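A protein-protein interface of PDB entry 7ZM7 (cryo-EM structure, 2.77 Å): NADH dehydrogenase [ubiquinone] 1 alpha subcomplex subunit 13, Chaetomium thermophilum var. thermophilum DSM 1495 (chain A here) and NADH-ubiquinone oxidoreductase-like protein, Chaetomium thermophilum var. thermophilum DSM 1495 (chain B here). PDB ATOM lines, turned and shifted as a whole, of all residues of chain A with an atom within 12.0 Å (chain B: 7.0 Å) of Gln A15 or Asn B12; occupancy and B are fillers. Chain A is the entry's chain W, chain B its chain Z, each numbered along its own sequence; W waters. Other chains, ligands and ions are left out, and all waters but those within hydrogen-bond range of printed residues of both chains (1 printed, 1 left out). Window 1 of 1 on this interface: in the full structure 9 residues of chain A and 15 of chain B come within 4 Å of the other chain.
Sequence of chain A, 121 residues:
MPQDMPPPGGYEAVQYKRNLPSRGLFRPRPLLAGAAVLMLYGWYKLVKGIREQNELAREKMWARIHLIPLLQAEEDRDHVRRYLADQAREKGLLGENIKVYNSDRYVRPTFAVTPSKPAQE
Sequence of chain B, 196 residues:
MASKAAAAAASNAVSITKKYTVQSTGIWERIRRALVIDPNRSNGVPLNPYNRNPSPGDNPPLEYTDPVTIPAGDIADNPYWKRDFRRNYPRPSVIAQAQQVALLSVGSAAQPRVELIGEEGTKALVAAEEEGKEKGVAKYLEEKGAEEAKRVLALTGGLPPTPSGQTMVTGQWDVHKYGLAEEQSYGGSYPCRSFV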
ATOM      1  N   TYR A  11     -10.808 -27.051  -6.357  1.00  0.00           N
ATOM      2  CA  TYR A  11     -11.948 -26.162  -6.419  1.00  0.00           C
ATOM      3  C   TYR A  11     -12.694 -26.196  -5.098  1.00  0.00           C
ATOM      4  O   TYR A  11     -12.627 -27.171  -4.349  1.00  0.00           O
ATOM      5  CB  TYR A  11     -12.878 -26.562  -7.560  1.00  0.00           C
ATOM      6  CG  TYR A  11     -12.368 -26.202  -8.927  1.00  0.00           C
ATOM      7  CD1 TYR A  11     -12.103 -24.900  -9.262  1.00  0.00           C
ATOM      8  CD2 TYR A  11     -12.159 -27.177  -9.883  1.00  0.00           C
ATOM      9  CE1 TYR A  11     -11.650 -24.569 -10.515  1.00  0.00           C
ATOM     10  CE2 TYR A  11     -11.705 -26.860 -11.136  1.00  0.00           C
ATOM     11  CZ  TYR A  11     -11.454 -25.553 -11.450  1.00  0.00           C
ATOM     12  OH  TYR A  11     -10.989 -25.215 -12.688  1.00  0.00           O
ATOM     13  N   GLU A  12     -13.394 -25.114  -4.804  1.00  0.00           N
ATOM     14  CA  GLU A  12     -14.195 -25.042  -3.597  1.00  0.00           C
ATOM     15  C   GLU A  12     -15.463 -25.883  -3.754  1.00  0.00           C
ATOM     16  O   GLU A  12     -15.831 -26.295  -4.852  1.00  0.00           O
ATOM     17  CB  GLU A  12     -14.510 -23.576  -3.278  1.00  0.00           C
ATOM     18  CG  GLU A  12     -15.282 -23.346  -2.004  1.00  0.00           C
ATOM     19  CD  GLU A  12     -14.642 -24.018  -0.807  1.00  0.00           C
ATOM     20  OE1 GLU A  12     -13.399 -23.981  -0.693  1.00  0.00           O
ATOM     21  OE2 GLU A  12     -15.388 -24.622  -0.005  1.00  0.00           O
ATOM     22  N   ALA A  13     -16.097 -26.191  -2.631  1.00  0.00           N
ATOM     23  CA  ALA A  13     -17.314 -26.984  -2.655  1.00  0.00           C
ATOM     24  C   ALA A  13     -18.470 -26.196  -3.254  1.00  0.00           C
ATOM     25  O   ALA A  13     -18.592 -24.989  -3.056  1.00  0.00           O
ATOM     26  CB  ALA A  13     -17.669 -27.447  -1.253  1.00  0.00           C
ATOM     27  N   VAL A  14     -19.317 -26.885  -3.996  1.00  0.00           N
ATOM     28  CA  VAL A  14     -20.497 -26.275  -4.560  1.00  0.00           C
ATOM     29  C   VAL A  14     -21.699 -26.678  -3.725  1.00  0.00           C
ATOM     30  O   VAL A  14     -21.661 -27.614  -2.925  1.00  0.00           O
ATOM     31  CB  VAL A  14     -20.702 -26.649  -6.045  1.00  0.00           C
ATOM     32  CG1 VAL A  14     -19.577 -26.098  -6.895  1.00  0.00           C
ATOM     33  CG2 VAL A  14     -20.825 -28.129  -6.202  1.00  0.00           C
ATOM     34  N   GLN A  15     -22.785 -25.947  -3.902  1.00  0.00           N
ATOM     35  CA  GLN A  15     -24.015 -26.236  -3.191  1.00  0.00           C
ATOM     36  C   GLN A  15     -24.761 -27.339  -3.924  1.00  0.00           C
ATOM     37  O   GLN A  15     -25.143 -27.169  -5.080  1.00  0.00           O
ATOM     38  CB  GLN A  15     -24.861 -24.972  -3.075  1.00  0.00           C
ATOM     39  CG  GLN A  15     -26.280 -25.231  -2.700  1.00  0.00           C
ATOM     40  CD  GLN A  15     -27.187 -24.064  -2.974  1.00  0.00           C
ATOM     41  OE1 GLN A  15     -26.796 -22.918  -2.841  1.00  0.00           O
ATOM     42  NE2 GLN A  15     -28.398 -24.355  -3.385  1.00  0.00           N
ATOM     43  N   TYR A  16     -24.977 -28.465  -3.255  1.00  0.00           N
ATOM     44  CA  TYR A  16     -25.693 -29.565  -3.867  1.00  0.00           C
ATOM     45  C   TYR A  16     -26.814 -30.150  -3.020  1.00  0.00           C
ATOM     46  O   TYR A  16     -27.586 -30.949  -3.546  1.00  0.00           O
ATOM     47  CB  TYR A  16     -24.718 -30.691  -4.271  1.00  0.00           C
ATOM     48  CG  TYR A  16     -24.208 -31.544  -3.146  1.00  0.00           C
ATOM     49  CD1 TYR A  16     -24.943 -32.624  -2.682  1.00  0.00           C
ATOM     50  CD2 TYR A  16     -22.976 -31.294  -2.564  1.00  0.00           C
ATOM     51  CE1 TYR A  16     -24.485 -33.405  -1.662  1.00  0.00           C
ATOM     52  CE2 TYR A  16     -22.512 -32.081  -1.543  1.00  0.00           C
ATOM     53  CZ  TYR A  16     -23.268 -33.132  -1.096  1.00  0.00           C
ATOM     54  OH  TYR A  16     -22.815 -33.917  -0.070  1.00  0.00           O
ATOM     55  N   LYS A  17     -26.945 -29.788  -1.753  1.00  0.00           N
ATOM     56  CA  LYS A  17     -28.002 -30.368  -0.942  1.00  0.00           C
ATOM     57  C   LYS A  17     -29.302 -29.588  -1.109  1.00  0.00           C
ATOM     58  O   LYS A  17     -29.314 -28.468  -1.614  1.00  0.00           O
ATOM     59  CB  LYS A  17     -27.599 -30.401   0.521  1.00  0.00           C
ATOM     60  CG  LYS A  17     -26.467 -31.313   0.870  1.00  0.00           C
ATOM     61  CD  LYS A  17     -26.230 -31.253   2.359  1.00  0.00           C
ATOM     62  CE  LYS A  17     -25.151 -32.201   2.814  1.00  0.00           C
ATOM     63  NZ  LYS A  17     -23.824 -31.781   2.308  1.00  0.00           N
ATOM     64  N   ARG A  18     -30.413 -30.194  -0.693  1.00  0.00           N
ATOM     65  CA  ARG A  18     -31.706 -29.530  -0.811  1.00  0.00           C
ATOM     66  C   ARG A  18     -31.716 -28.291   0.051  1.00  0.00           C
ATOM     67  O   ARG A  18     -31.559 -28.379   1.271  1.00  0.00           O
ATOM     68  CB  ARG A  18     -32.844 -30.436  -0.357  1.00  0.00           C
ATOM     69  CG  ARG A  18     -33.109 -31.636  -1.187  1.00  0.00           C
ATOM     70  CD  ARG A  18     -34.267 -32.406  -0.627  1.00  0.00           C
ATOM     71  NE  ARG A  18     -35.540 -31.782  -0.943  1.00  0.00           N
ATOM     72  CZ  ARG A  18     -36.457 -31.465  -0.041  1.00  0.00           C
ATOM     73  NH1 ARG A  18     -37.585 -30.905  -0.427  1.00  0.00           N
ATOM     74  NH2 ARG A  18     -36.240 -31.700   1.240  1.00  0.00           N
ATOM     75  N   ASN A  19     -31.927 -27.135  -0.563  1.00  0.00           N
ATOM     76  CA  ASN A  19     -31.931 -25.922   0.237  1.00  0.00           C
ATOM     77  C   ASN A  19     -33.342 -25.558   0.704  1.00  0.00           C
ATOM     78  O   ASN A  19     -33.637 -25.626   1.900  1.00  0.00           O
ATOM     79  CB  ASN A  19     -31.292 -24.790  -0.558  1.00  0.00           C
ATOM     80  CG  ASN A  19     -31.040 -23.592   0.278  1.00  0.00           C
ATOM     81  OD1 ASN A  19     -30.936 -23.692   1.488  1.00  0.00           O
ATOM     82  ND2 ASN A  19     -30.968 -22.435  -0.350  1.00  0.00           N
ATOM     83  N   LEU A  20     -34.216 -25.198  -0.224  1.00  0.00           N
ATOM     84  CA  LEU A  20     -35.662 -25.050  -0.040  1.00  0.00           C
ATOM     85  C   LEU A  20     -36.114 -24.348   1.235  1.00  0.00           C
ATOM     86  O   LEU A  20     -36.984 -24.881   1.926  1.00  0.00           O
ATOM     87  CB  LEU A  20     -36.330 -26.426  -0.023  1.00  0.00           C
ATOM     88  CG  LEU A  20     -36.649 -27.133  -1.329  1.00  0.00           C
ATOM     89  CD1 LEU A  20     -37.623 -26.300  -2.103  1.00  0.00           C
ATOM     90  CD2 LEU A  20     -35.417 -27.498  -2.121  1.00  0.00           C
ATOM     91  N   PRO A  21     -35.597 -23.146   1.614  1.00  0.00           N
ATOM     92  CA  PRO A  21     -35.874 -22.571   2.948  1.00  0.00           C
ATOM     93  C   PRO A  21     -37.249 -21.979   3.284  1.00  0.00           C
ATOM     94  O   PRO A  21     -37.659 -21.043   2.644  1.00  0.00           O
ATOM     95  CB  PRO A  21     -34.797 -21.491   3.092  1.00  0.00           C
ATOM     96  CG  PRO A  21     -34.596 -20.979   1.689  1.00  0.00           C
ATOM     97  CD  PRO A  21     -34.806 -22.186   0.804  1.00  0.00           C
ATOM     98  N   SER A  22     -37.869 -22.475   4.352  1.00  0.00           N
ATOM     99  CA  SER A  22     -39.205 -21.976   4.769  1.00  0.00           C
ATOM    100  C   SER A  22     -39.241 -20.456   4.931  1.00  0.00           C
ATOM    101  O   SER A  22     -38.341 -19.905   5.593  1.00  0.00           O
ATOM    102  CB  SER A  22     -39.703 -22.670   6.007  1.00  0.00           C
ATOM    103  OG  SER A  22     -41.009 -22.224   6.336  1.00  0.00           O
ATOM    104  N   SER B  11     -27.742 -23.455   6.825  1.00  0.00           N
ATOM    105  CA  SER B  11     -28.500 -24.334   5.945  1.00  0.00           C
ATOM    106  C   SER B  11     -27.592 -24.987   4.919  1.00  0.00           C
ATOM    107  O   SER B  11     -26.373 -25.011   5.077  1.00  0.00           O
ATOM    108  CB  SER B  11     -29.606 -23.562   5.228  1.00  0.00           C
ATOM    109  OG  SER B  11     -29.058 -22.645   4.299  1.00  0.00           O
ATOM    110  N   ASN B  12     -28.200 -25.513   3.858  1.00  0.00           N
ATOM    111  CA  ASN B  12     -27.439 -26.130   2.783  1.00  0.00           C
ATOM    112  C   ASN B  12     -26.942 -25.123   1.761  1.00  0.00           C
ATOM    113  O   ASN B  12     -26.150 -25.490   0.892  1.00  0.00           O
ATOM    114  CB  ASN B  12     -28.286 -27.184   2.071  1.00  0.00           C
ATOM    115  CG  ASN B  12     -28.600 -28.365   2.947  1.00  0.00           C
ATOM    116  OD1 ASN B  12     -27.787 -28.772   3.772  1.00  0.00           O
ATOM    117  ND2 ASN B  12     -29.788 -28.932   2.770  1.00  0.00           N
ATOM    118  N   ALA B  13     -27.378 -23.874   1.843  1.00  0.00           N
ATOM    119  CA  ALA B  13     -27.035 -22.901   0.828  1.00  0.00           C
ATOM    120  C   ALA B  13     -25.664 -22.304   1.086  1.00  0.00           C
ATOM    121  O   ALA B  13     -25.243 -22.155   2.234  1.00  0.00           O
ATOM    122  CB  ALA B  13     -28.075 -21.789   0.787  1.00  0.00           C
ATOM    123  N   VAL B  14     -24.971 -21.960   0.010  1.00  0.00           N
ATOM    124  CA  VAL B  14     -23.781 -21.147   0.092  1.00  0.00           C
ATOM    125  C   VAL B  14     -24.111 -19.791  -0.513  1.00  0.00           C
ATOM    126  O   VAL B  14     -25.039 -19.650  -1.313  1.00  0.00           O
ATOM    127  CB  VAL B  14     -22.563 -21.806  -0.595  1.00  0.00           C
ATOM    128  CG1 VAL B  14     -22.759 -21.919  -2.068  1.00  0.00           C
ATOM    129  CG2 VAL B  14     -21.283 -21.050  -0.263  1.00  0.00           C
ATOM    130  N   SER B  15     -23.355 -18.772  -0.105  1.00  0.00           N
ATOM    131  CA  SER B  15     -23.689 -17.395  -0.437  1.00  0.00           C
ATOM    132  C   SER B  15     -23.632 -17.135  -1.932  1.00  0.00           C
ATOM    133  O   SER B  15     -22.804 -17.696  -2.651  1.00  0.00           O
ATOM    134  CB  SER B  15     -22.748 -16.425   0.273  1.00  0.00           C
ATOM    135  OG  SER B  15     -23.034 -15.091  -0.110  1.00  0.00           O
ATOM    136  N   LYS B  19     -21.022 -17.595  -6.511  1.00  0.00           N
ATOM    137  CA  LYS B  19     -21.757 -18.508  -7.374  1.00  0.00           C
ATOM    138  C   LYS B  19     -21.587 -18.273  -8.867  1.00  0.00           C
ATOM    139  O   LYS B  19     -22.248 -18.960  -9.647  1.00  0.00           O
ATOM    140  CB  LYS B  19     -23.242 -18.498  -7.028  1.00  0.00           C
ATOM    141  CG  LYS B  19     -23.613 -19.549  -6.025  1.00  0.00           C
ATOM    142  CD  LYS B  19     -25.084 -19.581  -5.780  1.00  0.00           C
ATOM    143  CE  LYS B  19     -25.366 -20.379  -4.548  1.00  0.00           C
ATOM    144  NZ  LYS B  19     -26.784 -20.718  -4.458  1.00  0.00           N
ATOM    145  N   ASP B  38     -35.209 -17.124  -1.757  1.00  0.00           N
ATOM    146  CA  ASP B  38     -33.861 -17.423  -1.276  1.00  0.00           C
ATOM    147  C   ASP B  38     -32.892 -16.395  -1.830  1.00  0.00           C
ATOM    148  O   ASP B  38     -32.620 -16.397  -3.047  1.00  0.00           O
ATOM    149  CB  ASP B  38     -33.424 -18.833  -1.665  1.00  0.00           C
ATOM    150  CG  ASP B  38     -32.171 -19.277  -0.920  1.00  0.00           C
ATOM    151  OD1 ASP B  38     -31.758 -18.574   0.022  1.00  0.00           O
ATOM    152  OD2 ASP B  38     -31.585 -20.318  -1.280  1.00  0.00           O
ATOM    153  N   ASN B  40     -29.787 -16.325  -1.596  1.00  0.00           N
ATOM    154  CA  ASN B  40     -28.569 -16.970  -2.042  1.00  0.00           C
ATOM    155  C   ASN B  40     -28.724 -17.662  -3.382  1.00  0.00           C
ATOM    156  O   ASN B  40     -27.741 -18.171  -3.910  1.00  0.00           O
ATOM    157  CB  ASN B  40     -28.107 -17.967  -0.992  1.00  0.00           C
ATOM    158  CG  ASN B  40     -27.450 -17.300   0.177  1.00  0.00           C
ATOM    159  OD1 ASN B  40     -26.624 -16.415   0.018  1.00  0.00           O
ATOM    160  ND2 ASN B  40     -27.826 -17.712   1.371  1.00  0.00           N
ATOM    161  N   ARG B  41     -29.923 -17.700  -3.940  1.00  0.00           N
ATOM    162  CA  ARG B  41     -30.144 -18.335  -5.228  1.00  0.00           C
ATOM    163  C   ARG B  41     -29.631 -17.466  -6.359  1.00  0.00           C
ATOM    164  O   ARG B  41     -29.841 -16.256  -6.377  1.00  0.00           O
ATOM    165  CB  ARG B  41     -31.626 -18.614  -5.432  1.00  0.00           C
ATOM    166  CG  ARG B  41     -32.018 -20.010  -5.084  1.00  0.00           C
ATOM    167  CD  ARG B  41     -33.465 -20.241  -5.358  1.00  0.00           C
ATOM    168  NE  ARG B  41     -33.983 -21.328  -4.556  1.00  0.00           N
ATOM    169  CZ  ARG B  41     -35.251 -21.445  -4.198  1.00  0.00           C
ATOM    170  NH1 ARG B  41     -36.137 -20.547  -4.583  1.00  0.00           N
ATOM    171  NH2 ARG B  41     -35.626 -22.460  -3.452  1.00  0.00           N
ATOM    172  N   SER B  42     -28.959 -18.095  -7.301  1.00  0.00           N
ATOM    173  CA  SER B  42     -28.511 -17.457  -8.522  1.00  0.00           C
ATOM    174  C   SER B  42     -29.634 -17.421  -9.555  1.00  0.00           C
ATOM    175  O   SER B  42     -30.690 -18.030  -9.384  1.00  0.00           O
ATOM    176  CB  SER B  42     -27.298 -18.202  -9.047  1.00  0.00           C
ATOM    177  OG  SER B  42     -27.603 -19.561  -9.273  1.00  0.00           O
ATOM    178  N   GLU B 183     -26.603 -39.053   7.168  1.00  0.00           N
ATOM    179  CA  GLU B 183     -27.603 -37.997   7.128  1.00  0.00           C
ATOM    180  C   GLU B 183     -28.464 -38.176   5.889  1.00  0.00           C
ATOM    181  O   GLU B 183     -27.949 -38.295   4.780  1.00  0.00           O
ATOM    182  CB  GLU B 183     -26.940 -36.611   7.165  1.00  0.00           C
ATOM    183  CG  GLU B 183     -25.860 -36.380   6.119  1.00  0.00           C
ATOM    184  CD  GLU B 183     -26.405 -35.778   4.843  1.00  0.00           C
ATOM    185  OE1 GLU B 183     -27.485 -35.152   4.892  1.00  0.00           O
ATOM    186  OE2 GLU B 183     -25.760 -35.942   3.788  1.00  0.00           O
ATOM    187  N   SER B 185     -31.195 -37.196   3.009  1.00  0.00           N
ATOM    188  CA  SER B 185     -31.344 -35.977   2.236  1.00  0.00           C
ATOM    189  C   SER B 185     -32.740 -35.385   2.330  1.00  0.00           C
ATOM    190  O   SER B 185     -32.890 -34.165   2.284  1.00  0.00           O
ATOM    191  CB  SER B 185     -30.982 -36.254   0.789  1.00  0.00           C
ATOM    192  OG  SER B 185     -29.749 -36.937   0.688  1.00  0.00           O
HETATM  193  O   HOH W   1     -30.250 -33.036   0.756  1.00  0.00           O
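The side-chain amino group of Lys B19 lies within hydrogen-bond range of the side-chain amide oxygen of Gln A15 (2.7 Å). The backbone carbonyl oxygen of Arg A18 sits close to the side-chain amide nitrogen of Asn B12, 2.4 Å away. The side-chain amide nitrogen of Asn A19 lies close to the side-chain carboxylate of Asp B38.
The side-chain hydroxyl of Tyr A16 is in hydrogen-bond range of the side-chain amino group of Lys A17 (3.4 Å). N of Ala B13 sits at hydrogen-bond distance from OG of Ser B11, 3.2 Å away. NZ of Lys B19 sits at hydrogen-bond distance from O of Asn B40 (2.8 Å). The side-chain carboxylate of Asp B38 lies close to the backbone NH of Asn B40 (3.4 Å).
Among the printed residues, pairs that only touch across the chains: Asn A19 with Ala B13, Lys A17 with Asn B12, Gln A15 with Val B14, Asn A19 with Ser B11, Gln A15 with Asn B12, Arg A18 with Ser B185, Gln A15 with Ala B13, Lys A17 with Glu B183 and Pro A21 with Asp B38.
Of chain B, only Asn B12, Ala B13, Val B14 and Lys B19 come within 4 Å of Gln A15. Printed residues of chain A within 4 Å of Asn B12: Gln A15, Lys A17 and Arg A18. Of chain A, only Asn A19 comes within 4 Å of Ser B11. Of chain A, only Gln A15 and Asn A19 come within 4 Å of Ala B13. No residue of chain A comes within 4 Å of Asn B40. Of the printed residues of chain B, Pro A21 touches Asp B38. Of the printed residues of chain B, Lys A17 touches Asn B12 and Glu B183. Of the printed residues of chain A, Ser B185 touches Arg A18 (3.7 Å). Of the printed residues of chain A, Lys B19 touches Gln A15. Of the printed residues of chain B, Arg A18 touches Asn B12 (2.4 Å) and Ser B185 (3.7 Å). Val A14 touches none of the printed residues of chain B. The nearest residue of chain A that does not touch Asn B12 is Asn A19 (4.1 Å). The nearest printed residue of chain B that does not touch Pro A21 is Arg B41 (4.3 Å).
Of the 12 printed residues of chain B, 8 touch a printed residue of chain A. Hydrophobic or aromatic side chains of chain B within 4 Å of the printed part of chain A: Ala B13 and Val B14. Printed residues of chain A that touch a printed residue of chain B: Gln A15, Lys A17, Arg A18, Asn A19 and Pro A21. Among the printed residues, 12 pairs touch across the chains.
Water W1 lies within hydrogen-bond range of the backbone NH of Arg A18 (3.2 Å) and the backbone carbonyl oxygen of Ser B185 (3.3 Å).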
